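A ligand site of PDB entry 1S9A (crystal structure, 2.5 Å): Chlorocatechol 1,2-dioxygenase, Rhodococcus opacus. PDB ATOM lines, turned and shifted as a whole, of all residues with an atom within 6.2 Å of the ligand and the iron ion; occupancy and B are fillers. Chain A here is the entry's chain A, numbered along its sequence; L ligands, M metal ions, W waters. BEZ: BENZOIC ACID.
Within 4 Å of the iron ion: Tyr 134, Tyr 169, His 194 and His 196.
CD1 of Leu 49 touches C5 of the ligand (3.3 Å).
Asp 52 touches the ligand.
Ala 53 touches the ligand (N to C4, 3.5 Å).
CD1 of Ile 74 touches C2 of the ligand, 3.5 Å away.
CA of Gly 76 touches C2 of the ligand, at 3.6 Å.
CD of Pro 77 touches C6 of the ligand, at 3.5 Å.
Phe 78 touches the ligand (CD1 to O1, 3.7 Å).
SG of Cys 224 touches C4 of the ligand (3.5 Å).
Hydrophobic or aromatic side chains within 4 Å of the ligand: Leu 49, Ile 74, Pro 77, Phe 78, Tyr 134, Tyr 169, His 194 and His 196.
Within 4 Å of the ligand: Leu 49, Asp 52, Ala 53, Ile 74, Gly 76, Pro 77, Phe 78, Tyr 134, Tyr 169, Arg 191, His 194, His 196 and Cys 224.
The nearest printed residue that does not touch the ligand is Gln 210 (4.1 Å).
The guanidinium group (NH1) of Arg 191 lies close to an oxygen (O2) of the ligand (2.8 Å).
ND1 of His 194 sits close to NH1 of Arg 191.
N of His 196 is in hydrogen-bond range of O of Trp 126 (3.0 Å).
O of Tyr 169 is in hydrogen-bond range of N of Arg 191 (2.8 Å).
OE1 of Gln 210 sits at hydrogen-bond distance from NH1 of Arg 191 (2.6 Å).
The backbone carbonyl oxygen (O) of Ile 74 is in hydrogen-bond range of the side-chain amide nitrogen (NE2) of Gln 210 (2.9 Å).
The side-chain carboxylate (OE1) of Glu 56 sits at hydrogen-bond distance from the backbone NH (N) of Gly 76, 3.0 Å away.
The backbone carbonyl oxygen (O) of Phe 78 lies close to the indole nitrogen (NE1) of Trp 126 (3.5 Å).
The iron ion is bound by NE2 of His 194, O1 of the ligand, OH of Tyr 134, NE2 of His 196, OH of Tyr 169 and O2 of the ligand.
The iron ion has six donor atoms within binding distance.
Water W1 lies within hydrogen-bond range of N of Phe 78 (2.7 Å), O of Gln 75 (2.8 Å) and NE1 of Trp 126 (3.3 Å).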
ATOM      1  N   PRO A  48     -16.871 -12.537  27.283  1.00  0.00           N
ATOM      2  CA  PRO A  48     -18.210 -12.464  26.682  1.00  0.00           C
ATOM      3  C   PRO A  48     -18.900 -13.812  26.526  1.00  0.00           C
ATOM      4  O   PRO A  48     -20.003 -13.988  27.050  1.00  0.00           O
ATOM      5  CB  PRO A  48     -17.955 -11.833  25.316  1.00  0.00           C
ATOM      6  CG  PRO A  48     -16.770 -10.983  25.558  1.00  0.00           C
ATOM      7  CD  PRO A  48     -15.885 -11.777  26.483  1.00  0.00           C
ATOM      8  N   LEU A  49     -18.241 -14.756  25.849  1.00  0.00           N
ATOM      9  CA  LEU A  49     -18.771 -16.101  25.651  1.00  0.00           C
ATOM     10  C   LEU A  49     -19.100 -16.808  26.983  1.00  0.00           C
ATOM     11  O   LEU A  49     -20.178 -17.384  27.137  1.00  0.00           O
ATOM     12  CB  LEU A  49     -17.779 -16.943  24.828  1.00  0.00           C
ATOM     13  CG  LEU A  49     -17.858 -18.465  24.874  1.00  0.00           C
ATOM     14  CD1 LEU A  49     -19.029 -18.926  24.064  1.00  0.00           C
ATOM     15  CD2 LEU A  49     -16.591 -19.094  24.353  1.00  0.00           C
ATOM     16  N   TRP A  50     -18.172 -16.750  27.927  1.00  0.00           N
ATOM     17  CA  TRP A  50     -18.327 -17.372  29.237  1.00  0.00           C
ATOM     18  C   TRP A  50     -19.587 -16.819  29.937  1.00  0.00           C
ATOM     19  O   TRP A  50     -20.500 -17.586  30.274  1.00  0.00           O
ATOM     20  CB  TRP A  50     -17.083 -17.154  30.097  1.00  0.00           C
ATOM     21  CG  TRP A  50     -16.989 -18.112  31.241  1.00  0.00           C
ATOM     22  CD1 TRP A  50     -16.319 -19.297  31.250  1.00  0.00           C
ATOM     23  CD2 TRP A  50     -17.579 -17.977  32.538  1.00  0.00           C
ATOM     24  NE1 TRP A  50     -16.456 -19.918  32.476  1.00  0.00           N
ATOM     25  CE2 TRP A  50     -17.223 -19.124  33.277  1.00  0.00           C
ATOM     26  CE3 TRP A  50     -18.354 -16.983  33.155  1.00  0.00           C
ATOM     27  CZ2 TRP A  50     -17.627 -19.315  34.612  1.00  0.00           C
ATOM     28  CZ3 TRP A  50     -18.736 -17.172  34.490  1.00  0.00           C
ATOM     29  CH2 TRP A  50     -18.376 -18.332  35.194  1.00  0.00           C
ATOM     30  N   ASP A  52     -22.019 -14.919  28.938  1.00  0.00           N
ATOM     31  CA  ASP A  52     -23.228 -15.091  28.162  1.00  0.00           C
ATOM     32  C   ASP A  52     -23.721 -16.517  28.262  1.00  0.00           C
ATOM     33  O   ASP A  52     -24.937 -16.758  28.282  1.00  0.00           O
ATOM     34  CB  ASP A  52     -22.971 -14.730  26.695  1.00  0.00           C
ATOM     35  CG  ASP A  52     -22.926 -13.240  26.435  1.00  0.00           C
ATOM     36  OD1 ASP A  52     -23.265 -12.437  27.346  1.00  0.00           O
ATOM     37  OD2 ASP A  52     -22.571 -12.789  25.326  1.00  0.00           O
ATOM     38  N   ALA A  53     -22.783 -17.465  28.294  1.00  0.00           N
ATOM     39  CA  ALA A  53     -23.143 -18.889  28.339  1.00  0.00           C
ATOM     40  C   ALA A  53     -23.961 -19.165  29.579  1.00  0.00           C
ATOM     41  O   ALA A  53     -24.977 -19.837  29.516  1.00  0.00           O
ATOM     42  CB  ALA A  53     -21.908 -19.789  28.294  1.00  0.00           C
ATOM     43  N   PHE A  54     -23.540 -18.592  30.706  1.00  0.00           N
ATOM     44  CA  PHE A  54     -24.143 -18.911  31.998  1.00  0.00           C
ATOM     45  C   PHE A  54     -25.158 -17.910  32.522  1.00  0.00           C
ATOM     46  O   PHE A  54     -26.099 -18.304  33.209  1.00  0.00           O
ATOM     47  CB  PHE A  54     -23.066 -19.181  33.050  1.00  0.00           C
ATOM     48  CG  PHE A  54     -22.079 -20.240  32.638  1.00  0.00           C
ATOM     49  CD1 PHE A  54     -22.484 -21.556  32.485  1.00  0.00           C
ATOM     50  CD2 PHE A  54     -20.757 -19.916  32.393  1.00  0.00           C
ATOM     51  CE1 PHE A  54     -21.579 -22.548  32.108  1.00  0.00           C
ATOM     52  CE2 PHE A  54     -19.837 -20.895  31.996  1.00  0.00           C
ATOM     53  CZ  PHE A  54     -20.250 -22.218  31.853  1.00  0.00           C
ATOM     54  N   GLU A  56     -26.340 -14.477  30.778  1.00  0.00           N
ATOM     55  CA  GLU A  56     -27.191 -13.616  29.949  1.00  0.00           C
ATOM     56  C   GLU A  56     -28.663 -14.038  29.948  1.00  0.00           C
ATOM     57  O   GLU A  56     -29.548 -13.189  29.779  1.00  0.00           O
ATOM     58  CB  GLU A  56     -26.665 -13.526  28.509  1.00  0.00           C
ATOM     59  CG  GLU A  56     -27.161 -12.290  27.765  1.00  0.00           C
ATOM     60  CD  GLU A  56     -26.860 -12.344  26.282  1.00  0.00           C
ATOM     61  OE1 GLU A  56     -26.080 -13.211  25.843  1.00  0.00           O
ATOM     62  OE2 GLU A  56     -27.403 -11.504  25.531  1.00  0.00           O
ATOM     63  N   ILE A  74     -31.535 -14.292  24.562  1.00  0.00           N
ATOM     64  CA  ILE A  74     -30.195 -13.709  24.694  1.00  0.00           C
ATOM     65  C   ILE A  74     -29.596 -13.349  23.325  1.00  0.00           C
ATOM     66  O   ILE A  74     -29.964 -13.917  22.292  1.00  0.00           O
ATOM     67  CB  ILE A  74     -29.255 -14.628  25.548  1.00  0.00           C
ATOM     68  CG1 ILE A  74     -28.945 -15.978  24.840  1.00  0.00           C
ATOM     69  CG2 ILE A  74     -29.882 -14.872  26.906  1.00  0.00           C
ATOM     70  CD1 ILE A  74     -27.752 -16.780  25.436  1.00  0.00           C
ATOM     71  N   GLN A  75     -28.718 -12.360  23.312  1.00  0.00           N
ATOM     72  CA  GLN A  75     -28.050 -11.936  22.094  1.00  0.00           C
ATOM     73  C   GLN A  75     -26.833 -12.813  21.820  1.00  0.00           C
ATOM     74  O   GLN A  75     -26.439 -13.028  20.670  1.00  0.00           O
ATOM     75  CB  GLN A  75     -27.620 -10.479  22.241  1.00  0.00           C
ATOM     76  CG  GLN A  75     -26.905  -9.913  21.015  1.00  0.00           C
ATOM     77  CD  GLN A  75     -26.457  -8.491  21.196  1.00  0.00           C
ATOM     78  OE1 GLN A  75     -27.240  -7.644  21.610  1.00  0.00           O
ATOM     79  NE2 GLN A  75     -25.210  -8.212  20.875  1.00  0.00           N
ATOM     80  N   GLY A  76     -26.241 -13.333  22.890  1.00  0.00           N
ATOM     81  CA  GLY A  76     -24.946 -13.969  22.812  1.00  0.00           C
ATOM     82  C   GLY A  76     -23.862 -12.964  22.454  1.00  0.00           C
ATOM     83  O   GLY A  76     -24.150 -11.773  22.250  1.00  0.00           O
ATOM     84  N   PRO A  77     -22.623 -13.464  22.365  1.00  0.00           N
ATOM     85  CA  PRO A  77     -21.435 -12.637  22.070  1.00  0.00           C
ATOM     86  C   PRO A  77     -21.140 -12.385  20.587  1.00  0.00           C
ATOM     87  O   PRO A  77     -20.230 -11.613  20.291  1.00  0.00           O
ATOM     88  CB  PRO A  77     -20.300 -13.483  22.653  1.00  0.00           C
ATOM     89  CG  PRO A  77     -20.749 -14.900  22.396  1.00  0.00           C
ATOM     90  CD  PRO A  77     -22.253 -14.875  22.550  1.00  0.00           C
ATOM     91  N   PHE A  78     -21.878 -13.016  19.675  1.00  0.00           N
ATOM     92  CA  PHE A  78     -21.431 -13.042  18.283  1.00  0.00           C
ATOM     93  C   PHE A  78     -22.170 -12.111  17.324  1.00  0.00           C
ATOM     94  O   PHE A  78     -22.103 -12.288  16.121  1.00  0.00           O
ATOM     95  CB  PHE A  78     -21.392 -14.502  17.764  1.00  0.00           C
ATOM     96  CG  PHE A  78     -20.431 -15.369  18.517  1.00  0.00           C
ATOM     97  CD1 PHE A  78     -20.755 -16.684  18.824  1.00  0.00           C
ATOM     98  CD2 PHE A  78     -19.213 -14.869  18.941  1.00  0.00           C
ATOM     99  CE1 PHE A  78     -19.867 -17.482  19.532  1.00  0.00           C
ATOM    100  CE2 PHE A  78     -18.311 -15.663  19.651  1.00  0.00           C
ATOM    101  CZ  PHE A  78     -18.646 -16.961  19.951  1.00  0.00           C
ATOM    102  N   TRP A 126     -28.227 -12.850  12.034  1.00  0.00           N
ATOM    103  CA  TRP A 126     -26.950 -13.543  12.017  1.00  0.00           C
ATOM    104  C   TRP A 126     -27.124 -14.967  12.533  1.00  0.00           C
ATOM    105  O   TRP A 126     -28.052 -15.251  13.277  1.00  0.00           O
ATOM    106  CB  TRP A 126     -25.865 -12.778  12.774  1.00  0.00           C
ATOM    107  CG  TRP A 126     -25.944 -12.717  14.305  1.00  0.00           C
ATOM    108  CD1 TRP A 126     -25.099 -13.320  15.205  1.00  0.00           C
ATOM    109  CD2 TRP A 126     -26.867 -11.946  15.090  1.00  0.00           C
ATOM    110  NE1 TRP A 126     -25.455 -13.012  16.500  1.00  0.00           N
ATOM    111  CE2 TRP A 126     -26.536 -12.163  16.466  1.00  0.00           C
ATOM    112  CE3 TRP A 126     -27.956 -11.103  14.788  1.00  0.00           C
ATOM    113  CZ2 TRP A 126     -27.256 -11.566  17.512  1.00  0.00           C
ATOM    114  CZ3 TRP A 126     -28.670 -10.508  15.848  1.00  0.00           C
ATOM    115  CH2 TRP A 126     -28.312 -10.745  17.194  1.00  0.00           C
ATOM    116  N   HIS A 127     -26.277 -15.860  12.032  1.00  0.00           N
ATOM    117  CA  HIS A 127     -26.257 -17.250  12.473  1.00  0.00           C
ATOM    118  C   HIS A 127     -24.940 -17.927  12.110  1.00  0.00           C
ATOM    119  O   HIS A 127     -24.136 -17.377  11.371  1.00  0.00           O
ATOM    120  CB  HIS A 127     -27.474 -18.044  11.982  1.00  0.00           C
ATOM    121  CG  HIS A 127     -27.501 -18.309  10.505  1.00  0.00           C
ATOM    122  ND1 HIS A 127     -26.584 -19.116   9.872  1.00  0.00           N
ATOM    123  CD2 HIS A 127     -28.387 -17.927   9.559  1.00  0.00           C
ATOM    124  CE1 HIS A 127     -26.888 -19.192   8.589  1.00  0.00           C
ATOM    125  NE2 HIS A 127     -27.980 -18.491   8.369  1.00  0.00           N
ATOM    126  N   SER A 128     -24.707 -19.103  12.686  1.00  0.00           N
ATOM    127  CA  SER A 128     -23.469 -19.851  12.477  1.00  0.00           C
ATOM    128  C   SER A 128     -23.429 -20.520  11.106  1.00  0.00           C
ATOM    129  O   SER A 128     -24.477 -20.832  10.530  1.00  0.00           O
ATOM    130  CB  SER A 128     -23.347 -20.941  13.544  1.00  0.00           C
ATOM    131  OG  SER A 128     -24.408 -21.859  13.387  1.00  0.00           O
ATOM    132  N   TYR A 134     -18.994 -18.335  13.585  1.00  0.00           N
ATOM    133  CA  TYR A 134     -19.584 -17.042  13.258  1.00  0.00           C
ATOM    134  C   TYR A 134     -18.523 -16.155  12.622  1.00  0.00           C
ATOM    135  O   TYR A 134     -17.368 -16.079  13.090  1.00  0.00           O
ATOM    136  CB  TYR A 134     -20.151 -16.382  14.520  1.00  0.00           C
ATOM    137  CG  TYR A 134     -21.466 -16.945  15.014  1.00  0.00           C
ATOM    138  CD1 TYR A 134     -21.502 -17.944  15.982  1.00  0.00           C
ATOM    139  CD2 TYR A 134     -22.682 -16.463  14.535  1.00  0.00           C
ATOM    140  CE1 TYR A 134     -22.704 -18.444  16.452  1.00  0.00           C
ATOM    141  CE2 TYR A 134     -23.893 -16.953  15.004  1.00  0.00           C
ATOM    142  CZ  TYR A 134     -23.894 -17.960  15.956  1.00  0.00           C
ATOM    143  OH  TYR A 134     -25.099 -18.466  16.420  1.00  0.00           O
ATOM    144  N   TYR A 169     -24.668 -26.329  17.184  1.00  0.00           N
ATOM    145  CA  TYR A 169     -23.222 -26.099  17.237  1.00  0.00           C
ATOM    146  C   TYR A 169     -22.671 -26.171  18.643  1.00  0.00           C
ATOM    147  O   TYR A 169     -23.428 -26.098  19.614  1.00  0.00           O
ATOM    148  CB  TYR A 169     -22.804 -24.786  16.566  1.00  0.00           C
ATOM    149  CG  TYR A 169     -23.206 -23.502  17.271  1.00  0.00           C
ATOM    150  CD1 TYR A 169     -22.559 -23.075  18.446  1.00  0.00           C
ATOM    151  CD2 TYR A 169     -24.211 -22.702  16.751  1.00  0.00           C
ATOM    152  CE1 TYR A 169     -22.920 -21.905  19.094  1.00  0.00           C
ATOM    153  CE2 TYR A 169     -24.578 -21.523  17.380  1.00  0.00           C
ATOM    154  CZ  TYR A 169     -23.942 -21.130  18.547  1.00  0.00           C
ATOM    155  OH  TYR A 169     -24.338 -19.950  19.135  1.00  0.00           O
ATOM    156  N   ILE A 171     -19.738 -24.777  21.521  1.00  0.00           N
ATOM    157  CA  ILE A 171     -18.737 -23.857  22.018  1.00  0.00           C
ATOM    158  C   ILE A 171     -17.419 -24.626  22.027  1.00  0.00           C
ATOM    159  O   ILE A 171     -17.361 -25.753  22.537  1.00  0.00           O
ATOM    160  CB  ILE A 171     -19.140 -23.363  23.428  1.00  0.00           C
ATOM    161  CG1 ILE A 171     -20.210 -22.273  23.309  1.00  0.00           C
ATOM    162  CG2 ILE A 171     -17.930 -22.852  24.229  1.00  0.00           C
ATOM    163  CD1 ILE A 171     -21.222 -22.269  24.438  1.00  0.00           C
ATOM    164  N   ARG A 191     -25.370 -25.870  21.630  1.00  0.00           N
ATOM    165  CA  ARG A 191     -26.575 -25.063  21.533  1.00  0.00           C
ATOM    166  C   ARG A 191     -27.400 -25.694  20.425  1.00  0.00           C
ATOM    167  O   ARG A 191     -26.836 -26.188  19.458  1.00  0.00           O
ATOM    168  CB  ARG A 191     -26.249 -23.607  21.144  1.00  0.00           C
ATOM    169  CG  ARG A 191     -25.658 -22.693  22.250  1.00  0.00           C
ATOM    170  CD  ARG A 191     -26.249 -21.297  22.301  1.00  0.00           C
ATOM    171  NE  ARG A 191     -27.649 -21.384  22.666  1.00  0.00           N
ATOM    172  CZ  ARG A 191     -28.638 -20.634  22.179  1.00  0.00           C
ATOM    173  NH1 ARG A 191     -28.412 -19.687  21.287  1.00  0.00           N
ATOM    174  NH2 ARG A 191     -29.873 -20.848  22.597  1.00  0.00           N
ATOM    175  N   HIS A 194     -30.107 -22.160  15.683  1.00  0.00           N
ATOM    176  CA  HIS A 194     -30.867 -20.936  15.856  1.00  0.00           C
ATOM    177  C   HIS A 194     -30.457 -19.864  14.845  1.00  0.00           C
ATOM    178  O   HIS A 194     -29.268 -19.737  14.487  1.00  0.00           O
ATOM    179  CB  HIS A 194     -30.719 -20.398  17.284  1.00  0.00           C
ATOM    180  CG  HIS A 194     -29.293 -20.220  17.716  1.00  0.00           C
ATOM    181  ND1 HIS A 194     -28.591 -21.206  18.365  1.00  0.00           N
ATOM    182  CD2 HIS A 194     -28.450 -19.180  17.578  1.00  0.00           C
ATOM    183  CE1 HIS A 194     -27.364 -20.779  18.614  1.00  0.00           C
ATOM    184  NE2 HIS A 194     -27.251 -19.546  18.142  1.00  0.00           N
ATOM    185  N   HIS A 196     -30.346 -15.919  15.047  1.00  0.00           N
ATOM    186  CA  HIS A 196     -30.453 -14.721  15.880  1.00  0.00           C
ATOM    187  C   HIS A 196     -31.180 -13.637  15.132  1.00  0.00           C
ATOM    188  O   HIS A 196     -31.040 -13.503  13.905  1.00  0.00           O
ATOM    189  CB  HIS A 196     -29.096 -14.154  16.235  1.00  0.00           C
ATOM    190  CG  HIS A 196     -28.236 -15.060  17.054  1.00  0.00           C
ATOM    191  ND1 HIS A 196     -28.303 -15.096  18.427  1.00  0.00           N
ATOM    192  CD2 HIS A 196     -27.234 -15.901  16.705  1.00  0.00           C
ATOM    193  CE1 HIS A 196     -27.386 -15.938  18.892  1.00  0.00           C
ATOM    194  NE2 HIS A 196     -26.730 -16.442  17.862  1.00  0.00           N
ATOM    195  N   GLN A 210     -34.209 -15.104  19.191  1.00  0.00           N
ATOM    196  CA  GLN A 210     -33.641 -16.251  18.499  1.00  0.00           C
ATOM    197  C   GLN A 210     -34.792 -17.118  18.016  1.00  0.00           C
ATOM    198  O   GLN A 210     -35.828 -17.222  18.684  1.00  0.00           O
ATOM    199  CB  GLN A 210     -32.749 -17.069  19.425  1.00  0.00           C
ATOM    200  CG  GLN A 210     -31.542 -16.346  19.926  1.00  0.00           C
ATOM    201  CD  GLN A 210     -30.604 -17.239  20.714  1.00  0.00           C
ATOM    202  OE1 GLN A 210     -30.451 -18.491  20.310  1.00  0.00           O
ATOM    203  NE2 GLN A 210     -30.013 -16.790  21.700  1.00  0.00           N
ATOM    204  N   CYS A 224     -26.311 -23.147  27.039  1.00  0.00           N
ATOM    205  CA  CYS A 224     -26.384 -21.719  27.343  1.00  0.00           C
ATOM    206  C   CYS A 224     -27.684 -21.309  28.016  1.00  0.00           C
ATOM    207  O   CYS A 224     -27.827 -20.168  28.439  1.00  0.00           O
ATOM    208  CB  CYS A 224     -26.170 -20.924  26.065  1.00  0.00           C
ATOM    209  SG  CYS A 224     -24.433 -20.925  25.571  1.00  0.00           S
HETATM  210  C   BEZ L   1     -24.897 -17.837  21.026  1.00  0.00           C
HETATM  211  O1  BEZ L   1     -24.199 -17.566  19.820  1.00  0.00           O
HETATM  212  O2  BEZ L   1     -26.175 -18.052  20.945  1.00  0.00           O
HETATM  213  C1  BEZ L   1     -24.189 -17.866  22.342  1.00  0.00           C
HETATM  214  C2  BEZ L   1     -24.868 -17.473  23.497  1.00  0.00           C
HETATM  215  C3  BEZ L   1     -24.207 -17.479  24.721  1.00  0.00           C
HETATM  216  C4  BEZ L   1     -22.875 -17.885  24.799  1.00  0.00           C
HETATM  217  C5  BEZ L   1     -22.208 -18.291  23.648  1.00  0.00           C
HETATM  218  C6  BEZ L   1     -22.870 -18.277  22.418  1.00  0.00           C
HETATM  219 FE    FE M   1     -25.695 -18.284  18.513  1.00  0.00          FE
HETATM  220  O   HOH W   1     -24.317 -14.210  19.362  1.00  0.00           O
